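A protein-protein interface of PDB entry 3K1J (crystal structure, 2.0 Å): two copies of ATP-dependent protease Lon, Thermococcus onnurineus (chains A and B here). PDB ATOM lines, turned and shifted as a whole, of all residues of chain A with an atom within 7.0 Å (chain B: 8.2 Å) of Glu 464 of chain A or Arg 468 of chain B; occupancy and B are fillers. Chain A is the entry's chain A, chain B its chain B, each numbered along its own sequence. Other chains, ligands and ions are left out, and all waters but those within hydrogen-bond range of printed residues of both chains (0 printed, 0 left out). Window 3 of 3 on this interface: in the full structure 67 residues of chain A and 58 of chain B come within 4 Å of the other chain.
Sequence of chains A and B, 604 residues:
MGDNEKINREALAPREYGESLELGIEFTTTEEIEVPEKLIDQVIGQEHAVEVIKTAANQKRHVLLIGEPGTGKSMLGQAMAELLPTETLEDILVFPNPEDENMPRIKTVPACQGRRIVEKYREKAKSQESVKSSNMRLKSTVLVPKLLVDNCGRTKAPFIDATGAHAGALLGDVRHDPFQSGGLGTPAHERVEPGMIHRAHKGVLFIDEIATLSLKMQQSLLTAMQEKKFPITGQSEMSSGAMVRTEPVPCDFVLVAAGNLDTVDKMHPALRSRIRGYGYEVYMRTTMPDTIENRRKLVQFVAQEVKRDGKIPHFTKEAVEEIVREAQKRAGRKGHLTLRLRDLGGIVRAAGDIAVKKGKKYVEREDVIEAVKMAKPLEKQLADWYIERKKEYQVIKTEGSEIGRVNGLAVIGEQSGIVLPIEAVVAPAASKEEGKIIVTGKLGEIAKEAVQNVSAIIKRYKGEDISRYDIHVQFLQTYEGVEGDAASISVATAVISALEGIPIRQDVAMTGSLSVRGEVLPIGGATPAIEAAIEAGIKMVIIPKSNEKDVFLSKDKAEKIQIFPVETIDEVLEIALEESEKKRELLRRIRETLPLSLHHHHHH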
ATOM      1  N   LYS A 459     -13.271  13.586  31.767  1.00  0.00           N
ATOM      2  CA  LYS A 459     -13.621  14.696  30.901  1.00  0.00           C
ATOM      3  C   LYS A 459     -13.163  16.031  31.462  1.00  0.00           C
ATOM      4  O   LYS A 459     -12.704  16.895  30.719  1.00  0.00           O
ATOM      5  CB  LYS A 459     -15.127  14.725  30.672  1.00  0.00           C
ATOM      6  CG  LYS A 459     -15.625  13.564  29.848  1.00  0.00           C
ATOM      7  CD  LYS A 459     -17.055  13.787  29.411  1.00  0.00           C
ATOM      8  CE  LYS A 459     -18.027  13.083  30.311  1.00  0.00           C
ATOM      9  NZ  LYS A 459     -19.413  13.242  29.783  1.00  0.00           N
ATOM     10  N   ARG A 460     -13.280  16.204  32.774  1.00  0.00           N
ATOM     11  CA  ARG A 460     -12.878  17.465  33.383  1.00  0.00           C
ATOM     12  C   ARG A 460     -11.386  17.772  33.292  1.00  0.00           C
ATOM     13  O   ARG A 460     -11.013  18.880  32.928  1.00  0.00           O
ATOM     14  CB  ARG A 460     -13.333  17.532  34.846  1.00  0.00           C
ATOM     15  CG  ARG A 460     -14.784  17.985  35.006  1.00  0.00           C
ATOM     16  CD  ARG A 460     -15.297  17.761  36.429  1.00  0.00           C
ATOM     17  NE  ARG A 460     -14.578  18.570  37.409  1.00  0.00           N
ATOM     18  CZ  ARG A 460     -14.682  19.891  37.499  1.00  0.00           C
ATOM     19  NH1 ARG A 460     -15.475  20.548  36.664  1.00  0.00           N
ATOM     20  NH2 ARG A 460     -14.003  20.556  38.429  1.00  0.00           N
ATOM     21  N   LYS A 462      -9.160  16.275  31.260  1.00  0.00           N
ATOM     22  CA  LYS A 462      -8.720  16.174  29.876  1.00  0.00           C
ATOM     23  C   LYS A 462      -9.185  17.340  29.009  1.00  0.00           C
ATOM     24  O   LYS A 462      -8.489  17.743  28.081  1.00  0.00           O
ATOM     25  CB  LYS A 462      -9.194  14.848  29.279  1.00  0.00           C
ATOM     26  CG  LYS A 462      -8.868  14.654  27.809  1.00  0.00           C
ATOM     27  CD  LYS A 462      -7.408  14.956  27.484  1.00  0.00           C
ATOM     28  CE  LYS A 462      -6.443  14.104  28.285  1.00  0.00           C
ATOM     29  NZ  LYS A 462      -5.049  14.307  27.808  1.00  0.00           N
ATOM     30  N   GLY A 463     -10.363  17.878  29.305  1.00  0.00           N
ATOM     31  CA  GLY A 463     -10.865  19.002  28.539  1.00  0.00           C
ATOM     32  C   GLY A 463     -11.580  18.674  27.240  1.00  0.00           C
ATOM     33  O   GLY A 463     -11.840  17.516  26.911  1.00  0.00           O
ATOM     34  N   GLU A 464     -11.887  19.731  26.499  1.00  0.00           N
ATOM     35  CA  GLU A 464     -12.601  19.661  25.225  1.00  0.00           C
ATOM     36  C   GLU A 464     -12.183  18.576  24.241  1.00  0.00           C
ATOM     37  O   GLU A 464     -13.029  18.022  23.541  1.00  0.00           O
ATOM     38  CB  GLU A 464     -12.495  21.005  24.528  1.00  0.00           C
ATOM     39  CG  GLU A 464     -13.798  21.552  24.017  1.00  0.00           C
ATOM     40  CD  GLU A 464     -13.590  22.882  23.325  1.00  0.00           C
ATOM     41  OE1 GLU A 464     -13.040  23.798  23.979  1.00  0.00           O
ATOM     42  OE2 GLU A 464     -13.961  23.007  22.137  1.00  0.00           O
ATOM     43  N   ASP A 465     -10.886  18.286  24.171  1.00  0.00           N
ATOM     44  CA  ASP A 465     -10.386  17.269  23.250  1.00  0.00           C
ATOM     45  C   ASP A 465     -10.980  15.890  23.485  1.00  0.00           C
ATOM     46  O   ASP A 465     -10.970  15.038  22.594  1.00  0.00           O
ATOM     47  CB  ASP A 465      -8.860  17.158  23.339  1.00  0.00           C
ATOM     48  CG  ASP A 465      -8.152  18.353  22.735  1.00  0.00           C
ATOM     49  OD1 ASP A 465      -8.658  18.889  21.722  1.00  0.00           O
ATOM     50  OD2 ASP A 465      -7.085  18.746  23.264  1.00  0.00           O
ATOM     51  N   ILE A 466     -11.498  15.668  24.685  1.00  0.00           N
ATOM     52  CA  ILE A 466     -12.063  14.373  25.023  1.00  0.00           C
ATOM     53  C   ILE A 466     -13.060  13.878  23.978  1.00  0.00           C
ATOM     54  O   ILE A 466     -13.176  12.676  23.751  1.00  0.00           O
ATOM     55  CB  ILE A 466     -12.729  14.405  26.434  1.00  0.00           C
ATOM     56  CG1 ILE A 466     -13.068  12.983  26.877  1.00  0.00           C
ATOM     57  CG2 ILE A 466     -13.969  15.286  26.427  1.00  0.00           C
ATOM     58  CD1 ILE A 466     -11.843  12.124  27.117  1.00  0.00           C
ATOM     59  N   SER A 467     -13.754  14.797  23.317  1.00  0.00           N
ATOM     60  CA  SER A 467     -14.737  14.422  22.302  1.00  0.00           C
ATOM     61  C   SER A 467     -14.119  13.853  21.041  1.00  0.00           C
ATOM     62  O   SER A 467     -14.834  13.434  20.141  1.00  0.00           O
ATOM     63  CB  SER A 467     -15.582  15.634  21.921  1.00  0.00           C
ATOM     64  OG  SER A 467     -14.773  16.594  21.274  1.00  0.00           O
ATOM     65  N   ARG A 468     -12.794  13.861  20.991  1.00  0.00           N
ATOM     66  CA  ARG A 468     -12.062  13.376  19.837  1.00  0.00           C
ATOM     67  C   ARG A 468     -11.585  11.922  19.981  1.00  0.00           C
ATOM     68  O   ARG A 468     -10.994  11.358  19.052  1.00  0.00           O
ATOM     69  CB  ARG A 468     -10.873  14.308  19.621  1.00  0.00           C
ATOM     70  CG  ARG A 468      -9.972  14.011  18.460  1.00  0.00           C
ATOM     71  CD  ARG A 468      -8.874  15.054  18.430  1.00  0.00           C
ATOM     72  NE  ARG A 468      -7.981  14.931  17.281  1.00  0.00           N
ATOM     73  CZ  ARG A 468      -6.978  15.774  17.039  1.00  0.00           C
ATOM     74  NH1 ARG A 468      -6.748  16.795  17.867  1.00  0.00           N
ATOM     75  NH2 ARG A 468      -6.210  15.604  15.967  1.00  0.00           N
ATOM     76  N   VAL B 426     -19.541  19.803  36.635  1.00  0.00           N
ATOM     77  CA  VAL B 426     -19.734  20.217  35.268  1.00  0.00           C
ATOM     78  C   VAL B 426     -18.502  19.812  34.464  1.00  0.00           C
ATOM     79  O   VAL B 426     -17.366  20.030  34.891  1.00  0.00           O
ATOM     80  CB  VAL B 426     -19.950  21.750  35.212  1.00  0.00           C
ATOM     81  CG1 VAL B 426     -19.961  22.232  33.786  1.00  0.00           C
ATOM     82  CG2 VAL B 426     -21.276  22.103  35.881  1.00  0.00           C
ATOM     83  N   ALA B 427     -18.729  19.206  33.306  1.00  0.00           N
ATOM     84  CA  ALA B 427     -17.629  18.782  32.462  1.00  0.00           C
ATOM     85  C   ALA B 427     -17.894  19.204  31.028  1.00  0.00           C
ATOM     86  O   ALA B 427     -19.013  19.567  30.678  1.00  0.00           O
ATOM     87  CB  ALA B 427     -17.481  17.276  32.531  1.00  0.00           C
ATOM     88  N   PRO B 428     -16.855  19.169  30.180  1.00  0.00           N
ATOM     89  CA  PRO B 428     -16.991  19.538  28.768  1.00  0.00           C
ATOM     90  C   PRO B 428     -17.882  18.479  28.133  1.00  0.00           C
ATOM     91  O   PRO B 428     -17.745  17.299  28.450  1.00  0.00           O
ATOM     92  CB  PRO B 428     -15.555  19.442  28.243  1.00  0.00           C
ATOM     93  CG  PRO B 428     -14.715  19.681  29.463  1.00  0.00           C
ATOM     94  CD  PRO B 428     -15.446  18.901  30.523  1.00  0.00           C
ATOM     95  N   ALA B 429     -18.788  18.872  27.242  1.00  0.00           N
ATOM     96  CA  ALA B 429     -19.667  17.882  26.616  1.00  0.00           C
ATOM     97  C   ALA B 429     -18.876  16.849  25.813  1.00  0.00           C
ATOM     98  O   ALA B 429     -17.916  17.187  25.124  1.00  0.00           O
ATOM     99  CB  ALA B 429     -20.690  18.575  25.711  1.00  0.00           C
ATOM    100  N   ALA B 430     -19.281  15.588  25.896  1.00  0.00           N
ATOM    101  CA  ALA B 430     -18.599  14.529  25.161  1.00  0.00           C
ATOM    102  C   ALA B 430     -18.977  14.609  23.678  1.00  0.00           C
ATOM    103  O   ALA B 430     -18.246  14.140  22.805  1.00  0.00           O
ATOM    104  CB  ALA B 430     -18.978  13.163  25.735  1.00  0.00           C
ATOM    105  N   SER B 431     -20.128  15.209  23.410  1.00  0.00           N
ATOM    106  CA  SER B 431     -20.610  15.368  22.054  1.00  0.00           C
ATOM    107  C   SER B 431     -20.650  16.843  21.709  1.00  0.00           C
ATOM    108  O   SER B 431     -21.226  17.645  22.437  1.00  0.00           O
ATOM    109  CB  SER B 431     -22.007  14.782  21.914  1.00  0.00           C
ATOM    110  OG  SER B 431     -22.645  15.335  20.783  1.00  0.00           O
ATOM    111  N   LYS B 432     -20.042  17.204  20.590  1.00  0.00           N
ATOM    112  CA  LYS B 432     -20.016  18.600  20.180  1.00  0.00           C
ATOM    113  C   LYS B 432     -21.364  19.067  19.627  1.00  0.00           C
ATOM    114  O   LYS B 432     -21.536  20.242  19.321  1.00  0.00           O
ATOM    115  CB  LYS B 432     -18.891  18.814  19.158  1.00  0.00           C
ATOM    116  CG  LYS B 432     -18.911  17.826  18.001  1.00  0.00           C
ATOM    117  CD  LYS B 432     -17.520  17.619  17.391  1.00  0.00           C
ATOM    118  CE  LYS B 432     -16.573  16.952  18.384  1.00  0.00           C
ATOM    119  NZ  LYS B 432     -15.323  16.450  17.740  1.00  0.00           N
ATOM    120  N   GLU B 433     -22.328  18.154  19.541  1.00  0.00           N
ATOM    121  CA  GLU B 433     -23.657  18.481  19.024  1.00  0.00           C
ATOM    122  C   GLU B 433     -24.687  18.767  20.118  1.00  0.00           C
ATOM    123  O   GLU B 433     -25.634  19.538  19.920  1.00  0.00           O
ATOM    124  CB  GLU B 433     -24.159  17.348  18.136  1.00  0.00           C
ATOM    125  N   GLU B 434     -24.507  18.152  21.276  1.00  0.00           N
ATOM    126  CA  GLU B 434     -25.458  18.341  22.355  1.00  0.00           C
ATOM    127  C   GLU B 434     -24.828  18.191  23.734  1.00  0.00           C
ATOM    128  O   GLU B 434     -23.906  17.409  23.930  1.00  0.00           O
ATOM    129  CB  GLU B 434     -26.615  17.339  22.194  1.00  0.00           C
ATOM    130  CG  GLU B 434     -27.297  16.975  23.494  1.00  0.00           C
ATOM    131  CD  GLU B 434     -28.405  15.938  23.336  1.00  0.00           C
ATOM    132  OE1 GLU B 434     -28.246  14.990  22.524  1.00  0.00           O
ATOM    133  OE2 GLU B 434     -29.428  16.072  24.050  1.00  0.00           O
ATOM    134  N   GLY B 435     -25.336  18.959  24.686  1.00  0.00           N
ATOM    135  CA  GLY B 435     -24.845  18.869  26.044  1.00  0.00           C
ATOM    136  C   GLY B 435     -25.848  17.990  26.755  1.00  0.00           C
ATOM    137  O   GLY B 435     -27.032  17.993  26.397  1.00  0.00           O
ATOM    138  N   LYS B 436     -25.403  17.238  27.754  1.00  0.00           N
ATOM    139  CA  LYS B 436     -26.311  16.354  28.468  1.00  0.00           C
ATOM    140  C   LYS B 436     -26.225  16.479  29.979  1.00  0.00           C
ATOM    141  O   LYS B 436     -25.275  17.042  30.526  1.00  0.00           O
ATOM    142  CB  LYS B 436     -26.023  14.899  28.088  1.00  0.00           C
ATOM    143  CG  LYS B 436     -26.211  14.578  26.623  1.00  0.00           C
ATOM    144  CD  LYS B 436     -25.772  13.169  26.346  1.00  0.00           C
ATOM    145  CE  LYS B 436     -25.845  12.828  24.866  1.00  0.00           C
ATOM    146  NZ  LYS B 436     -25.309  11.458  24.616  1.00  0.00           N
ATOM    147  N   GLY B 463     -29.261  29.489  29.452  1.00  0.00           N
ATOM    148  CA  GLY B 463     -29.123  29.863  28.055  1.00  0.00           C
ATOM    149  C   GLY B 463     -28.432  28.826  27.184  1.00  0.00           C
ATOM    150  O   GLY B 463     -28.158  27.710  27.623  1.00  0.00           O
ATOM    151  N   GLU B 464     -28.135  29.214  25.945  1.00  0.00           N
ATOM    152  CA  GLU B 464     -27.502  28.331  24.962  1.00  0.00           C
ATOM    153  C   GLU B 464     -26.188  27.669  25.345  1.00  0.00           C
ATOM    154  O   GLU B 464     -25.868  26.598  24.830  1.00  0.00           O
ATOM    155  CB  GLU B 464     -27.309  29.070  23.638  1.00  0.00           C
ATOM    156  CG  GLU B 464     -28.575  29.213  22.833  1.00  0.00           C
ATOM    157  CD  GLU B 464     -28.934  30.658  22.574  1.00  0.00           C
ATOM    158  OE1 GLU B 464     -29.103  31.416  23.559  1.00  0.00           O
ATOM    159  OE2 GLU B 464     -29.046  31.035  21.388  1.00  0.00           O
ATOM    160  N   ASP B 465     -25.416  28.291  26.226  1.00  0.00           N
ATOM    161  CA  ASP B 465     -24.148  27.705  26.642  1.00  0.00           C
ATOM    162  C   ASP B 465     -24.340  26.296  27.200  1.00  0.00           C
ATOM    163  O   ASP B 465     -23.446  25.453  27.119  1.00  0.00           O
ATOM    164  CB  ASP B 465     -23.488  28.586  27.707  1.00  0.00           C
ATOM    165  CG  ASP B 465     -22.769  29.783  27.112  1.00  0.00           C
ATOM    166  OD1 ASP B 465     -23.045  30.129  25.941  1.00  0.00           O
ATOM    167  OD2 ASP B 465     -21.931  30.380  27.820  1.00  0.00           O
ATOM    168  N   ILE B 466     -25.519  26.043  27.752  1.00  0.00           N
ATOM    169  CA  ILE B 466     -25.816  24.750  28.353  1.00  0.00           C
ATOM    170  C   ILE B 466     -25.489  23.543  27.467  1.00  0.00           C
ATOM    171  O   ILE B 466     -25.143  22.473  27.980  1.00  0.00           O
ATOM    172  CB  ILE B 466     -27.302  24.677  28.788  1.00  0.00           C
ATOM    173  CG1 ILE B 466     -27.515  23.478  29.711  1.00  0.00           C
ATOM    174  CG2 ILE B 466     -28.198  24.565  27.577  1.00  0.00           C
ATOM    175  CD1 ILE B 466     -26.688  23.534  30.978  1.00  0.00           C
ATOM    176  N   SER B 467     -25.590  23.706  26.150  1.00  0.00           N
ATOM    177  CA  SER B 467     -25.312  22.598  25.235  1.00  0.00           C
ATOM    178  C   SER B 467     -23.829  22.278  25.112  1.00  0.00           C
ATOM    179  O   SER B 467     -23.447  21.279  24.500  1.00  0.00           O
ATOM    180  CB  SER B 467     -25.868  22.920  23.844  1.00  0.00           C
ATOM    181  OG  SER B 467     -25.190  24.018  23.278  1.00  0.00           O
ATOM    182  N   ARG B 468     -23.016  23.141  25.704  1.00  0.00           N
ATOM    183  CA  ARG B 468     -21.570  23.017  25.657  1.00  0.00           C
ATOM    184  C   ARG B 468     -21.034  22.157  26.825  1.00  0.00           C
ATOM    185  O   ARG B 468     -19.837  21.825  26.856  1.00  0.00           O
ATOM    186  CB  ARG B 468     -20.952  24.401  25.742  1.00  0.00           C
ATOM    187  CG  ARG B 468     -19.466  24.466  25.545  1.00  0.00           C
ATOM    188  CD  ARG B 468     -19.057  25.859  25.138  1.00  0.00           C
ATOM    189  NE  ARG B 468     -17.815  25.829  24.374  1.00  0.00           N
ATOM    190  CZ  ARG B 468     -17.653  25.141  23.246  1.00  0.00           C
ATOM    191  NH1 ARG B 468     -18.658  24.428  22.750  1.00  0.00           N
ATOM    192  NH2 ARG B 468     -16.483  25.158  22.619  1.00  0.00           N
ATOM    193  N   TYR B 469     -21.918  21.738  27.741  1.00  0.00           N
ATOM    194  CA  TYR B 469     -21.492  20.942  28.885  1.00  0.00           C
ATOM    195  C   TYR B 469     -22.291  19.684  29.090  1.00  0.00           C
ATOM    196  O   TYR B 469     -23.403  19.514  28.622  1.00  0.00           O
ATOM    197  CB  TYR B 469     -21.605  21.758  30.178  1.00  0.00           C
ATOM    198  CG  TYR B 469     -20.816  23.037  30.213  1.00  0.00           C
ATOM    199  CD1 TYR B 469     -19.433  23.042  30.005  1.00  0.00           C
ATOM    200  CD2 TYR B 469     -21.451  24.240  30.467  1.00  0.00           C
ATOM    201  CE1 TYR B 469     -18.702  24.242  30.050  1.00  0.00           C
ATOM    202  CE2 TYR B 469     -20.735  25.443  30.518  1.00  0.00           C
ATOM    203  CZ  TYR B 469     -19.366  25.417  30.304  1.00  0.00           C
ATOM    204  OH  TYR B 469     -18.618  26.577  30.322  1.00  0.00           O
ATOM    205  N   ASP B 470     -21.629  18.809  29.818  1.00  0.00           N
ATOM    206  CA  ASP B 470     -22.159  17.560  30.270  1.00  0.00           C
ATOM    207  C   ASP B 470     -22.149  17.768  31.784  1.00  0.00           C
ATOM    208  O   ASP B 470     -21.089  17.994  32.383  1.00  0.00           O
ATOM    209  CB  ASP B 470     -21.260  16.361  29.904  1.00  0.00           C
ATOM    210  CG  ASP B 470     -21.629  15.726  28.583  1.00  0.00           C
ATOM    211  OD1 ASP B 470     -22.642  16.130  27.999  1.00  0.00           O
ATOM    212  OD2 ASP B 470     -20.912  14.806  28.138  1.00  0.00           O
ATOM    213  N   ILE B 471     -23.324  17.687  32.394  1.00  0.00           N
ATOM    214  CA  ILE B 471     -23.447  17.862  33.827  1.00  0.00           C
ATOM    215  C   ILE B 471     -23.662  16.472  34.426  1.00  0.00           C
ATOM    216  O   ILE B 471     -24.612  15.778  34.072  1.00  0.00           O
ATOM    217  CB  ILE B 471     -24.646  18.761  34.147  1.00  0.00           C
ATOM    218  CG1 ILE B 471     -24.476  20.110  33.449  1.00  0.00           C
ATOM    219  CG2 ILE B 471     -24.780  18.944  35.650  1.00  0.00           C
ATOM    220  CD1 ILE B 471     -25.669  21.039  33.586  1.00  0.00           C
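OE2 of Glu 464 of chain A lies within salt-bridge range of NH2 of Arg 468 of chain B, 3.3 Å away. O of Val 426 of chain B is in hydrogen-bond range of NH1 of Arg 460 of chain A. The side-chain amino group (NZ) of Lys 459 of chain A is in salt-bridge range of the side-chain carboxylate (OD2) of Asp 470 of chain B (2.7 Å).
The backbone NH of Ala 427 of chain B sits at hydrogen-bond distance from the backbone carbonyl oxygen of Asp 470 of chain B (2.8 Å). The backbone carbonyl oxygen (O) of Glu 464 of chain A sits at hydrogen-bond distance from the side-chain hydroxyl (OG) of Ser 467 of chain A. OD2 of Asp 470 of chain B lies within hydrogen-bond range of N of Ala 430 of chain B, 2.9 Å away. The backbone NH (N) of Lys 436 of chain B lies within hydrogen-bond range of the side-chain carboxylate (OD1) of Asp 470 of chain B (3.0 Å). The backbone NH (N) of Ala 429 of chain B lies within hydrogen-bond range of the backbone carbonyl oxygen (O) of Arg 468 of chain B (3.2 Å).
Lys 459 of chain A touches Ala 427 of chain B (CB to CB, 3.9 Å). Pro 428 of chain B touches Lys 459 of chain A. Arg 460 of chain A touches Ala 427 of chain B (CG to CB, 3.7 Å). Gly 463 of chain A touches Pro 428 of chain B (C to CG, 3.97 Å). Ala 430 of chain B touches Ser 467 of chain A (O to CB, 3.2 Å). Ser 467 of chain A touches Lys 432 of chain B (OG to CE, 3.4 Å).
Printed residues of chain B within 4 Å of Lys 459 of chain A: Ala 427 (3.9 Å), Pro 428 (3.4 Å) and Asp 470 (2.7 Å). Gly 463 of chain A touches just one residue of chain B: Pro 428. Of chain B, only Arg 468 (3.3 Å) comes within 4 Å of Glu 464 of chain A. Of the printed residues of chain A, Lys 432 of chain B touches Ser 467. Of chain A, only Glu 464 comes within 4 Å of Arg 468 of chain B. Printed residues of chain A within 4 Å of Asp 470 of chain B: Lys 459. The nearest residue of chain B that does not touch Glu 464 of chain A is Pro 428 of chain B (4.1 Å). The nearest printed residue of chain A that does not touch Arg 468 of chain B is Ile 466 of chain A (8.8 Å). The nearest printed residue of chain B that does not touch Ser 467 of chain A is Ala 429 of chain B (4.3 Å).
Of the 20 printed residues of chain B, 7 touch a printed residue of chain A. Printed residues of chain B that touch a printed residue of chain A: Val 426, Ala 427, Pro 428, Ala 430, Lys 432, Arg 468 and Asp 470. Hydrophobic or aromatic side chains of chain B within 4 Å of the printed part of chain A: Ala 427 and Pro 428.
Glu 464 of chain A touches Arg 468 of chain B, but with the chains exchanged Arg 468 of chain A does not touch Glu 464 of chain B (18.7 Å). 6 positions are printed for both chains. Of the 9 pairs that touch across the chains among the printed residues, none has its exchanged pair printed and touching as well.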
